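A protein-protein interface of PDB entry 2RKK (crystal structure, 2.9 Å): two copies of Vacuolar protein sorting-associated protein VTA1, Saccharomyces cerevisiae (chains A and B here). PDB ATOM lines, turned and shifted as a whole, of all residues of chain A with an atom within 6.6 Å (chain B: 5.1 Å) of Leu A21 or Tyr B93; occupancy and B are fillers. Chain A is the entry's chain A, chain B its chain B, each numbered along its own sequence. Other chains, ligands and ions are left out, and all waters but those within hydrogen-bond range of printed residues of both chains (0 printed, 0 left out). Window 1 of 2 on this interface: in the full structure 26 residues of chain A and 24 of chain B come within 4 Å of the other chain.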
ATOM      1  N   ASP A  15      22.912  -1.317 -22.582  1.00  0.00           N
ATOM      2  CA  ASP A  15      21.814  -1.816 -23.387  1.00  0.00           C
ATOM      3  C   ASP A  15      22.142  -3.214 -23.893  1.00  0.00           C
ATOM      4  O   ASP A  15      21.294  -4.097 -23.870  1.00  0.00           O
ATOM      5  CB  ASP A  15      21.541  -0.863 -24.541  1.00  0.00           C
ATOM      6  CG  ASP A  15      20.557   0.219 -24.157  1.00  0.00           C
ATOM      7  OD1 ASP A  15      20.648   0.713 -23.004  1.00  0.00           O
ATOM      8  OD2 ASP A  15      19.690   0.578 -24.987  1.00  0.00           O
ATOM      9  N   PHE A  16      23.376  -3.415 -24.340  1.00  0.00           N
ATOM     10  CA  PHE A  16      23.778  -4.723 -24.824  1.00  0.00           C
ATOM     11  C   PHE A  16      23.763  -5.796 -23.752  1.00  0.00           C
ATOM     12  O   PHE A  16      23.647  -6.988 -24.065  1.00  0.00           O
ATOM     13  CB  PHE A  16      25.167  -4.683 -25.423  1.00  0.00           C
ATOM     14  CG  PHE A  16      25.186  -4.286 -26.852  1.00  0.00           C
ATOM     15  CD1 PHE A  16      25.048  -2.964 -27.215  1.00  0.00           C
ATOM     16  CD2 PHE A  16      25.345  -5.236 -27.844  1.00  0.00           C
ATOM     17  CE1 PHE A  16      25.083  -2.591 -28.552  1.00  0.00           C
ATOM     18  CE2 PHE A  16      25.380  -4.870 -29.184  1.00  0.00           C
ATOM     19  CZ  PHE A  16      25.248  -3.550 -29.533  1.00  0.00           C
ATOM     20  N   ASP A  17      23.927  -5.403 -22.494  1.00  0.00           N
ATOM     21  CA  ASP A  17      23.894  -6.395 -21.424  1.00  0.00           C
ATOM     22  C   ASP A  17      22.448  -6.765 -21.155  1.00  0.00           C
ATOM     23  O   ASP A  17      22.079  -7.946 -21.136  1.00  0.00           O
ATOM     24  CB  ASP A  17      24.540  -5.870 -20.129  1.00  0.00           C
ATOM     25  CG  ASP A  17      26.065  -5.782 -20.222  1.00  0.00           C
ATOM     26  OD1 ASP A  17      26.739  -6.818 -20.468  1.00  0.00           O
ATOM     27  OD2 ASP A  17      26.595  -4.670 -20.038  1.00  0.00           O
ATOM     28  N   LYS A  18      21.622  -5.744 -20.968  1.00  0.00           N
ATOM     29  CA  LYS A  18      20.213  -5.968 -20.687  1.00  0.00           C
ATOM     30  C   LYS A  18      19.506  -6.831 -21.741  1.00  0.00           C
ATOM     31  O   LYS A  18      18.476  -7.444 -21.453  1.00  0.00           O
ATOM     32  CB  LYS A  18      19.504  -4.627 -20.533  1.00  0.00           C
ATOM     33  CG  LYS A  18      18.044  -4.754 -20.183  1.00  0.00           C
ATOM     34  CD  LYS A  18      17.413  -3.381 -19.996  1.00  0.00           C
ATOM     35  CE  LYS A  18      15.888  -3.475 -19.919  1.00  0.00           C
ATOM     36  NZ  LYS A  18      15.256  -3.886 -21.213  1.00  0.00           N
ATOM     37  N   VAL A  19      20.066  -6.886 -22.949  1.00  0.00           N
ATOM     38  CA  VAL A  19      19.483  -7.678 -24.027  1.00  0.00           C
ATOM     39  C   VAL A  19      20.137  -9.055 -24.088  1.00  0.00           C
ATOM     40  O   VAL A  19      19.642  -9.961 -24.757  1.00  0.00           O
ATOM     41  CB  VAL A  19      19.649  -6.961 -25.396  1.00  0.00           C
ATOM     42  CG1 VAL A  19      21.098  -6.986 -25.824  1.00  0.00           C
ATOM     43  CG2 VAL A  19      18.758  -7.604 -26.438  1.00  0.00           C
ATOM     44  N   GLY A  20      21.257  -9.205 -23.387  1.00  0.00           N
ATOM     45  CA  GLY A  20      21.950 -10.484 -23.351  1.00  0.00           C
ATOM     46  C   GLY A  20      23.077 -10.734 -24.332  1.00  0.00           C
ATOM     47  O   GLY A  20      23.154 -11.807 -24.939  1.00  0.00           O
ATOM     48  N   LEU A  21      23.957  -9.748 -24.487  1.00  0.00           N
ATOM     49  CA  LEU A  21      25.104  -9.868 -25.389  1.00  0.00           C
ATOM     50  C   LEU A  21      26.366  -9.575 -24.592  1.00  0.00           C
ATOM     51  O   LEU A  21      27.337  -9.026 -25.109  1.00  0.00           O
ATOM     52  CB  LEU A  21      24.960  -8.889 -26.548  1.00  0.00           C
ATOM     53  CG  LEU A  21      23.809  -9.219 -27.509  1.00  0.00           C
ATOM     54  CD1 LEU A  21      23.655  -8.110 -28.553  1.00  0.00           C
ATOM     55  CD2 LEU A  21      24.088 -10.556 -28.172  1.00  0.00           C
ATOM     56  N   GLY A  22      26.321  -9.962 -23.317  1.00  0.00           N
ATOM     57  CA  GLY A  22      27.413  -9.749 -22.373  1.00  0.00           C
ATOM     58  C   GLY A  22      28.837  -9.561 -22.849  1.00  0.00           C
ATOM     59  O   GLY A  22      29.526  -8.656 -22.375  1.00  0.00           O
ATOM     60  N   ILE A  23      29.296 -10.422 -23.748  1.00  0.00           N
ATOM     61  CA  ILE A  23      30.648 -10.283 -24.227  1.00  0.00           C
ATOM     62  C   ILE A  23      30.819  -8.963 -24.984  1.00  0.00           C
ATOM     63  O   ILE A  23      31.828  -8.259 -24.816  1.00  0.00           O
ATOM     64  CB  ILE A  23      31.055 -11.453 -25.131  1.00  0.00           C
ATOM     65  CG1 ILE A  23      31.240 -12.725 -24.280  1.00  0.00           C
ATOM     66  CG2 ILE A  23      32.359 -11.128 -25.849  1.00  0.00           C
ATOM     67  CD1 ILE A  23      31.715 -13.945 -25.073  1.00  0.00           C
ATOM     68  N   ILE A  24      29.841  -8.616 -25.813  1.00  0.00           N
ATOM     69  CA  ILE A  24      29.907  -7.363 -26.561  1.00  0.00           C
ATOM     70  C   ILE A  24      29.976  -6.198 -25.554  1.00  0.00           C
ATOM     71  O   ILE A  24      30.940  -5.433 -25.557  1.00  0.00           O
ATOM     72  CB  ILE A  24      28.654  -7.149 -27.482  1.00  0.00           C
ATOM     73  CG1 ILE A  24      28.333  -8.412 -28.289  1.00  0.00           C
ATOM     74  CG2 ILE A  24      28.927  -6.039 -28.467  1.00  0.00           C
ATOM     75  CD1 ILE A  24      29.344  -8.750 -29.346  1.00  0.00           C
ATOM     76  N   GLY A  25      28.962  -6.086 -24.696  1.00  0.00           N
ATOM     77  CA  GLY A  25      28.925  -5.012 -23.721  1.00  0.00           C
ATOM     78  C   GLY A  25      30.149  -4.995 -22.834  1.00  0.00           C
ATOM     79  O   GLY A  25      30.523  -3.952 -22.285  1.00  0.00           O
ATOM     80  N   TYR A  26      30.772  -6.161 -22.678  1.00  0.00           N
ATOM     81  CA  TYR A  26      31.974  -6.274 -21.860  1.00  0.00           C
ATOM     82  C   TYR A  26      33.040  -5.366 -22.464  1.00  0.00           C
ATOM     83  O   TYR A  26      33.520  -4.429 -21.826  1.00  0.00           O
ATOM     84  CB  TYR A  26      32.469  -7.722 -21.861  1.00  0.00           C
ATOM     85  CG  TYR A  26      33.856  -7.916 -21.282  1.00  0.00           C
ATOM     86  CD1 TYR A  26      34.108  -7.694 -19.908  1.00  0.00           C
ATOM     87  CD2 TYR A  26      34.903  -8.388 -22.093  1.00  0.00           C
ATOM     88  CE1 TYR A  26      35.366  -7.951 -19.350  1.00  0.00           C
ATOM     89  CE2 TYR A  26      36.161  -8.647 -21.557  1.00  0.00           C
ATOM     90  CZ  TYR A  26      36.390  -8.433 -20.181  1.00  0.00           C
ATOM     91  OH  TYR A  26      37.626  -8.723 -19.636  1.00  0.00           O
ATOM     92  N   PHE A  60      32.698  -9.563 -14.409  1.00  0.00           N
ATOM     93  CA  PHE A  60      32.368 -10.316 -15.612  1.00  0.00           C
ATOM     94  C   PHE A  60      33.396 -11.369 -15.992  1.00  0.00           C
ATOM     95  O   PHE A  60      33.046 -12.525 -16.237  1.00  0.00           O
ATOM     96  CB  PHE A  60      32.185  -9.380 -16.809  1.00  0.00           C
ATOM     97  CG  PHE A  60      31.760 -10.089 -18.061  1.00  0.00           C
ATOM     98  CD1 PHE A  60      30.423 -10.160 -18.403  1.00  0.00           C
ATOM     99  CD2 PHE A  60      32.700 -10.716 -18.881  1.00  0.00           C
ATOM    100  CE1 PHE A  60      30.015 -10.842 -19.540  1.00  0.00           C
ATOM    101  CE2 PHE A  60      32.309 -11.407 -20.028  1.00  0.00           C
ATOM    102  CZ  PHE A  60      30.962 -11.470 -20.359  1.00  0.00           C
ATOM    103  N   TYR A  93      35.530 -12.116 -33.180  1.00  0.00           N
ATOM    104  CA  TYR A  93      34.117 -12.294 -32.845  1.00  0.00           C
ATOM    105  C   TYR A  93      33.448 -10.925 -32.854  1.00  0.00           C
ATOM    106  O   TYR A  93      32.360 -10.745 -33.405  1.00  0.00           O
ATOM    107  CB  TYR A  93      33.929 -12.940 -31.466  1.00  0.00           C
ATOM    108  CG  TYR A  93      32.484 -12.970 -31.002  1.00  0.00           C
ATOM    109  CD1 TYR A  93      31.529 -13.768 -31.648  1.00  0.00           C
ATOM    110  CD2 TYR A  93      32.069 -12.178 -29.934  1.00  0.00           C
ATOM    111  CE1 TYR A  93      30.184 -13.777 -31.235  1.00  0.00           C
ATOM    112  CE2 TYR A  93      30.743 -12.170 -29.511  1.00  0.00           C
ATOM    113  CZ  TYR A  93      29.800 -12.967 -30.158  1.00  0.00           C
ATOM    114  OH  TYR A  93      28.484 -12.923 -29.709  1.00  0.00           O
ATOM    115  N   PHE A  97      30.352  -9.713 -35.507  1.00  0.00           N
ATOM    116  CA  PHE A  97      29.075  -9.235 -35.009  1.00  0.00           C
ATOM    117  C   PHE A  97      28.800  -7.815 -35.513  1.00  0.00           C
ATOM    118  O   PHE A  97      27.746  -7.553 -36.109  1.00  0.00           O
ATOM    119  CB  PHE A  97      29.045  -9.229 -33.486  1.00  0.00           C
ATOM    120  CG  PHE A  97      27.859  -8.500 -32.921  1.00  0.00           C
ATOM    121  CD1 PHE A  97      26.679  -9.182 -32.625  1.00  0.00           C
ATOM    122  CD2 PHE A  97      27.902  -7.119 -32.744  1.00  0.00           C
ATOM    123  CE1 PHE A  97      25.555  -8.502 -32.166  1.00  0.00           C
ATOM    124  CE2 PHE A  97      26.790  -6.425 -32.288  1.00  0.00           C
ATOM    125  CZ  PHE A  97      25.611  -7.122 -31.995  1.00  0.00           C
ATOM    126  N   SER A 100      28.000  -7.660 -39.250  1.00  0.00           N
ATOM    127  CA  SER A 100      26.673  -8.100 -39.658  1.00  0.00           C
ATOM    128  C   SER A 100      25.645  -7.005 -39.386  1.00  0.00           C
ATOM    129  O   SER A 100      24.703  -6.798 -40.161  1.00  0.00           O
ATOM    130  CB  SER A 100      26.313  -9.399 -38.939  1.00  0.00           C
ATOM    131  OG  SER A 100      27.187 -10.447 -39.353  1.00  0.00           O
ATOM    132  N   GLY B  20      26.963 -14.447 -20.262  1.00  0.00           N
ATOM    133  CA  GLY B  20      26.503 -13.165 -20.767  1.00  0.00           C
ATOM    134  C   GLY B  20      25.778 -13.279 -22.098  1.00  0.00           C
ATOM    135  O   GLY B  20      25.079 -12.355 -22.510  1.00  0.00           O
ATOM    136  N   LEU B  21      25.947 -14.412 -22.773  1.00  0.00           N
ATOM    137  CA  LEU B  21      25.295 -14.626 -24.050  1.00  0.00           C
ATOM    138  C   LEU B  21      23.842 -15.007 -23.826  1.00  0.00           C
ATOM    139  O   LEU B  21      23.479 -16.183 -23.878  1.00  0.00           O
ATOM    140  CB  LEU B  21      25.993 -15.730 -24.842  1.00  0.00           C
ATOM    141  CG  LEU B  21      27.501 -15.578 -25.026  1.00  0.00           C
ATOM    142  CD1 LEU B  21      27.839 -14.162 -25.493  1.00  0.00           C
ATOM    143  CD2 LEU B  21      28.179 -15.876 -23.709  1.00  0.00           C
ATOM    144  N   GLY B  22      23.018 -13.999 -23.553  1.00  0.00           N
ATOM    145  CA  GLY B  22      21.606 -14.233 -23.321  1.00  0.00           C
ATOM    146  C   GLY B  22      20.875 -14.596 -24.600  1.00  0.00           C
ATOM    147  O   GLY B  22      19.863 -15.299 -24.559  1.00  0.00           O
ATOM    148  N   ILE B  23      21.377 -14.113 -25.733  1.00  0.00           N
ATOM    149  CA  ILE B  23      20.736 -14.425 -26.998  1.00  0.00           C
ATOM    150  C   ILE B  23      20.903 -15.899 -27.305  1.00  0.00           C
ATOM    151  O   ILE B  23      19.948 -16.570 -27.695  1.00  0.00           O
ATOM    152  CB  ILE B  23      21.307 -13.606 -28.164  1.00  0.00           C
ATOM    153  CG1 ILE B  23      20.810 -12.167 -28.069  1.00  0.00           C
ATOM    154  CG2 ILE B  23      20.862 -14.198 -29.497  1.00  0.00           C
ATOM    155  CD1 ILE B  23      19.312 -12.024 -28.109  1.00  0.00           C
ATOM    156  N   ILE B  24      22.109 -16.417 -27.116  1.00  0.00           N
ATOM    157  CA  ILE B  24      22.318 -17.828 -27.389  1.00  0.00           C
ATOM    158  C   ILE B  24      21.469 -18.658 -26.431  1.00  0.00           C
ATOM    159  O   ILE B  24      20.793 -19.601 -26.851  1.00  0.00           O
ATOM    160  CB  ILE B  24      23.825 -18.227 -27.300  1.00  0.00           C
ATOM    161  CG1 ILE B  24      24.557 -17.798 -28.580  1.00  0.00           C
ATOM    162  CG2 ILE B  24      23.974 -19.741 -27.209  1.00  0.00           C
ATOM    163  CD1 ILE B  24      25.054 -16.368 -28.588  1.00  0.00           C
ATOM    164  N   MET B  80      19.652  -3.929 -30.938  1.00  0.00           N
ATOM    165  CA  MET B  80      19.918  -5.331 -31.215  1.00  0.00           C
ATOM    166  C   MET B  80      18.743  -6.281 -31.036  1.00  0.00           C
ATOM    167  O   MET B  80      18.892  -7.483 -31.227  1.00  0.00           O
ATOM    168  CB  MET B  80      21.093  -5.810 -30.368  1.00  0.00           C
ATOM    169  CG  MET B  80      22.426  -5.584 -31.048  1.00  0.00           C
ATOM    170  SD  MET B  80      22.492  -6.410 -32.659  1.00  0.00           S
ATOM    171  CE  MET B  80      22.273  -5.028 -33.808  1.00  0.00           C
ATOM    172  N   LEU B  83      17.229  -9.131 -33.286  1.00  0.00           N
ATOM    173  CA  LEU B  83      17.667 -10.523 -33.280  1.00  0.00           C
ATOM    174  C   LEU B  83      16.560 -11.465 -32.854  1.00  0.00           C
ATOM    175  O   LEU B  83      16.464 -12.577 -33.356  1.00  0.00           O
ATOM    176  CB  LEU B  83      18.844 -10.669 -32.327  1.00  0.00           C
ATOM    177  CG  LEU B  83      20.048 -11.386 -32.912  1.00  0.00           C
ATOM    178  CD1 LEU B  83      20.250 -11.060 -34.400  1.00  0.00           C
ATOM    179  CD2 LEU B  83      21.238 -10.966 -32.083  1.00  0.00           C
ATOM    180  N   LYS B  89      18.538 -13.008 -39.417  1.00  0.00           N
ATOM    181  CA  LYS B  89      19.610 -12.409 -38.646  1.00  0.00           C
ATOM    182  C   LYS B  89      19.969 -13.338 -37.506  1.00  0.00           C
ATOM    183  O   LYS B  89      21.139 -13.706 -37.338  1.00  0.00           O
ATOM    184  CB  LYS B  89      19.169 -11.057 -38.095  1.00  0.00           C
ATOM    185  CG  LYS B  89      19.010 -10.009 -39.171  1.00  0.00           C
ATOM    186  CD  LYS B  89      18.468  -8.727 -38.596  1.00  0.00           C
ATOM    187  CE  LYS B  89      17.971  -7.805 -39.696  1.00  0.00           C
ATOM    188  NZ  LYS B  89      17.254  -6.630 -39.122  1.00  0.00           N
ATOM    189  N   ALA B  90      18.957 -13.716 -36.727  1.00  0.00           N
ATOM    190  CA  ALA B  90      19.153 -14.626 -35.600  1.00  0.00           C
ATOM    191  C   ALA B  90      20.010 -15.815 -36.043  1.00  0.00           C
ATOM    192  O   ALA B  90      20.936 -16.210 -35.345  1.00  0.00           O
ATOM    193  CB  ALA B  90      17.820 -15.105 -35.087  1.00  0.00           C
ATOM    194  N   LYS B  91      19.716 -16.358 -37.219  1.00  0.00           N
ATOM    195  CA  LYS B  91      20.474 -17.488 -37.719  1.00  0.00           C
ATOM    196  C   LYS B  91      21.919 -17.097 -37.996  1.00  0.00           C
ATOM    197  O   LYS B  91      22.843 -17.883 -37.786  1.00  0.00           O
ATOM    198  CB  LYS B  91      19.836 -18.029 -38.991  1.00  0.00           C
ATOM    199  CG  LYS B  91      20.458 -19.303 -39.513  1.00  0.00           C
ATOM    200  CD  LYS B  91      19.783 -19.739 -40.799  1.00  0.00           C
ATOM    201  CE  LYS B  91      20.363 -19.004 -42.004  1.00  0.00           C
ATOM    202  NZ  LYS B  91      19.550 -19.251 -43.234  1.00  0.00           N
ATOM    203  N   ILE B  92      22.111 -15.872 -38.466  1.00  0.00           N
ATOM    204  CA  ILE B  92      23.440 -15.365 -38.764  1.00  0.00           C
ATOM    205  C   ILE B  92      24.309 -15.307 -37.507  1.00  0.00           C
ATOM    206  O   ILE B  92      25.351 -15.945 -37.437  1.00  0.00           O
ATOM    207  CB  ILE B  92      23.333 -13.970 -39.397  1.00  0.00           C
ATOM    208  CG1 ILE B  92      22.651 -14.107 -40.756  1.00  0.00           C
ATOM    209  CG2 ILE B  92      24.712 -13.314 -39.498  1.00  0.00           C
ATOM    210  CD1 ILE B  92      22.465 -12.813 -41.495  1.00  0.00           C
ATOM    211  N   TYR B  93      23.865 -14.542 -36.521  1.00  0.00           N
ATOM    212  CA  TYR B  93      24.599 -14.403 -35.285  1.00  0.00           C
ATOM    213  C   TYR B  93      24.736 -15.742 -34.581  1.00  0.00           C
ATOM    214  O   TYR B  93      25.648 -15.937 -33.783  1.00  0.00           O
ATOM    215  CB  TYR B  93      23.893 -13.419 -34.376  1.00  0.00           C
ATOM    216  CG  TYR B  93      24.372 -13.466 -32.947  1.00  0.00           C
ATOM    217  CD1 TYR B  93      25.567 -12.842 -32.550  1.00  0.00           C
ATOM    218  CD2 TYR B  93      23.616 -14.136 -31.972  1.00  0.00           C
ATOM    219  CE1 TYR B  93      25.980 -12.887 -31.203  1.00  0.00           C
ATOM    220  CE2 TYR B  93      24.024 -14.184 -30.637  1.00  0.00           C
ATOM    221  CZ  TYR B  93      25.196 -13.561 -30.252  1.00  0.00           C
ATOM    222  OH  TYR B  93      25.531 -13.604 -28.930  1.00  0.00           O
ATOM    223  N   MET B  94      23.832 -16.669 -34.875  1.00  0.00           N
ATOM    224  CA  MET B  94      23.855 -18.003 -34.272  1.00  0.00           C
ATOM    225  C   MET B  94      24.961 -18.832 -34.911  1.00  0.00           C
ATOM    226  O   MET B  94      25.747 -19.471 -34.220  1.00  0.00           O
ATOM    227  CB  MET B  94      22.509 -18.693 -34.500  1.00  0.00           C
ATOM    228  CG  MET B  94      22.234 -19.879 -33.603  1.00  0.00           C
ATOM    229  SD  MET B  94      21.909 -19.383 -31.909  1.00  0.00           S
ATOM    230  CE  MET B  94      22.155 -20.947 -31.044  1.00  0.00           C
ATOM    231  N   LEU B  95      25.027 -18.821 -36.237  1.00  0.00           N
ATOM    232  CA  LEU B  95      26.050 -19.592 -36.924  1.00  0.00           C
ATOM    233  C   LEU B  95      27.444 -19.037 -36.677  1.00  0.00           C
ATOM    234  O   LEU B  95      28.362 -19.798 -36.413  1.00  0.00           O
ATOM    235  CB  LEU B  95      25.762 -19.643 -38.417  1.00  0.00           C
ATOM    236  CG  LEU B  95      26.277 -20.924 -39.062  1.00  0.00           C
ATOM    237  CD1 LEU B  95      25.815 -22.138 -38.286  1.00  0.00           C
ATOM    238  CD2 LEU B  95      25.777 -20.988 -40.480  1.00  0.00           C
ATOM    239  N   ASN B  96      27.600 -17.719 -36.764  1.00  0.00           N
ATOM    240  CA  ASN B  96      28.891 -17.083 -36.523  1.00  0.00           C
ATOM    241  C   ASN B  96      29.463 -17.625 -35.215  1.00  0.00           C
ATOM    242  O   ASN B  96      30.564 -18.169 -35.186  1.00  0.00           O
ATOM    243  CB  ASN B  96      28.715 -15.557 -36.428  1.00  0.00           C
ATOM    244  CG  ASN B  96      30.006 -14.817 -36.015  1.00  0.00           C
ATOM    245  OD1 ASN B  96      29.961 -13.644 -35.607  1.00  0.00           O
ATOM    246  ND2 ASN B  96      31.153 -15.494 -36.128  1.00  0.00           N
ATOM    247  N   PHE B  97      28.692 -17.486 -34.143  1.00  0.00           N
ATOM    248  CA  PHE B  97      29.095 -17.943 -32.824  1.00  0.00           C
ATOM    249  C   PHE B  97      29.452 -19.428 -32.792  1.00  0.00           C
ATOM    250  O   PHE B  97      30.534 -19.794 -32.348  1.00  0.00           O
ATOM    251  CB  PHE B  97      27.969 -17.686 -31.837  1.00  0.00           C
ATOM    252  CG  PHE B  97      28.347 -17.911 -30.410  1.00  0.00           C
ATOM    253  CD1 PHE B  97      28.904 -16.886 -29.658  1.00  0.00           C
ATOM    254  CD2 PHE B  97      28.130 -19.139 -29.805  1.00  0.00           C
ATOM    255  CE1 PHE B  97      29.221 -17.068 -28.308  1.00  0.00           C
ATOM    256  CE2 PHE B  97      28.444 -19.334 -28.456  1.00  0.00           C
ATOM    257  CZ  PHE B  97      28.995 -18.296 -27.711  1.00  0.00           C
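The backbone NH (N) of Leu A21 lies within hydrogen-bond range of the backbone carbonyl oxygen (O) of Gly B20 (3.5 Å). The backbone carbonyl oxygen of Gly A20 sits at hydrogen-bond distance from the backbone NH of Gly B22 (2.6 Å). The side-chain hydroxyl (OH) of Tyr B93 sits close to the side-chain hydroxyl (OH) of Tyr A93 (3.1 Å). The backbone carbonyl oxygen (O) of Gly A20 is in hydrogen-bond range of the backbone NH (N) of Ile B23, 3.0 Å away. O of Gly A20 lies close to O of Gly B20 (3.1 Å). O of Gly B20 is in hydrogen-bond range of N of Gly A22, 2.8 Å away.
The backbone carbonyl oxygen (O) of Phe A16 sits at hydrogen-bond distance from the backbone NH (N) of Leu A21 (2.8 Å).
CE2 of Phe A16 touches CG of Met B80, at 3.6 Å. Val A19 touches Ile B23. O of Gly A20 touches C of Leu B21, 3.5 Å away. Leu A21 touches Ile B23 (CD2 to CG1, 3.7 Å). Met B80 touches Leu A21. CD2 of Leu A21 touches OH of Tyr B93, 3.5 Å away. Tyr A93 touches Phe B97 (CE1 to CD1, 3.7 Å). SD of Met B80 touches CZ of Phe A97 (3.3 Å). Phe A97 touches Tyr B93. OG of Ser A100 touches CG2 of Ile B92, 3.8 Å away.
Of chain B, only Gly B20, Ile B23, Met B80 and Tyr B93 come within 4 Å of Leu A21. Tyr B93 touches three residues of chain A. Of the printed residues of chain B, Phe A16 touches Met B80. Printed residues of chain A within 4 Å of Met B80: Phe A16, Leu A21 and Phe A97. Of the printed residues of chain B, Gly A22 touches Gly B20. Of the printed residues of chain A, Ile B92 touches Ser A100 (3.8 Å). Lys B89 touches none of the printed residues of chain A. The nearest residue of chain B that does not touch Leu A21 is Gly B22 (4.5 Å).
Printed residues of chain B that touch a printed residue of chain A: Gly B20, Leu B21, Gly B22, Ile B23, Met B80, Ile B92, Tyr B93, Asn B96 and Phe B97. Along chain A the printed residues that touch a printed residue of chain B span positions 16 to 100. Among the printed residues, 18 pairs touch across the chains. Among the printed residues, no Asp or Glu carboxylate lies within 4 Å of a Lys or Arg side-chain nitrogen of the other chain.
Gly A20 touches Leu B21, and with the chains exchanged Leu A21 touches Gly B20. Gly A20 touches Gly B22, and with the chains exchanged Gly A22 touches Gly B20. Leu A21 touches Tyr B93, but with the chains exchanged Tyr A93 does not touch Leu B21 (4.4 Å). Tyr B93 touches its own counterpart, Tyr A93.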
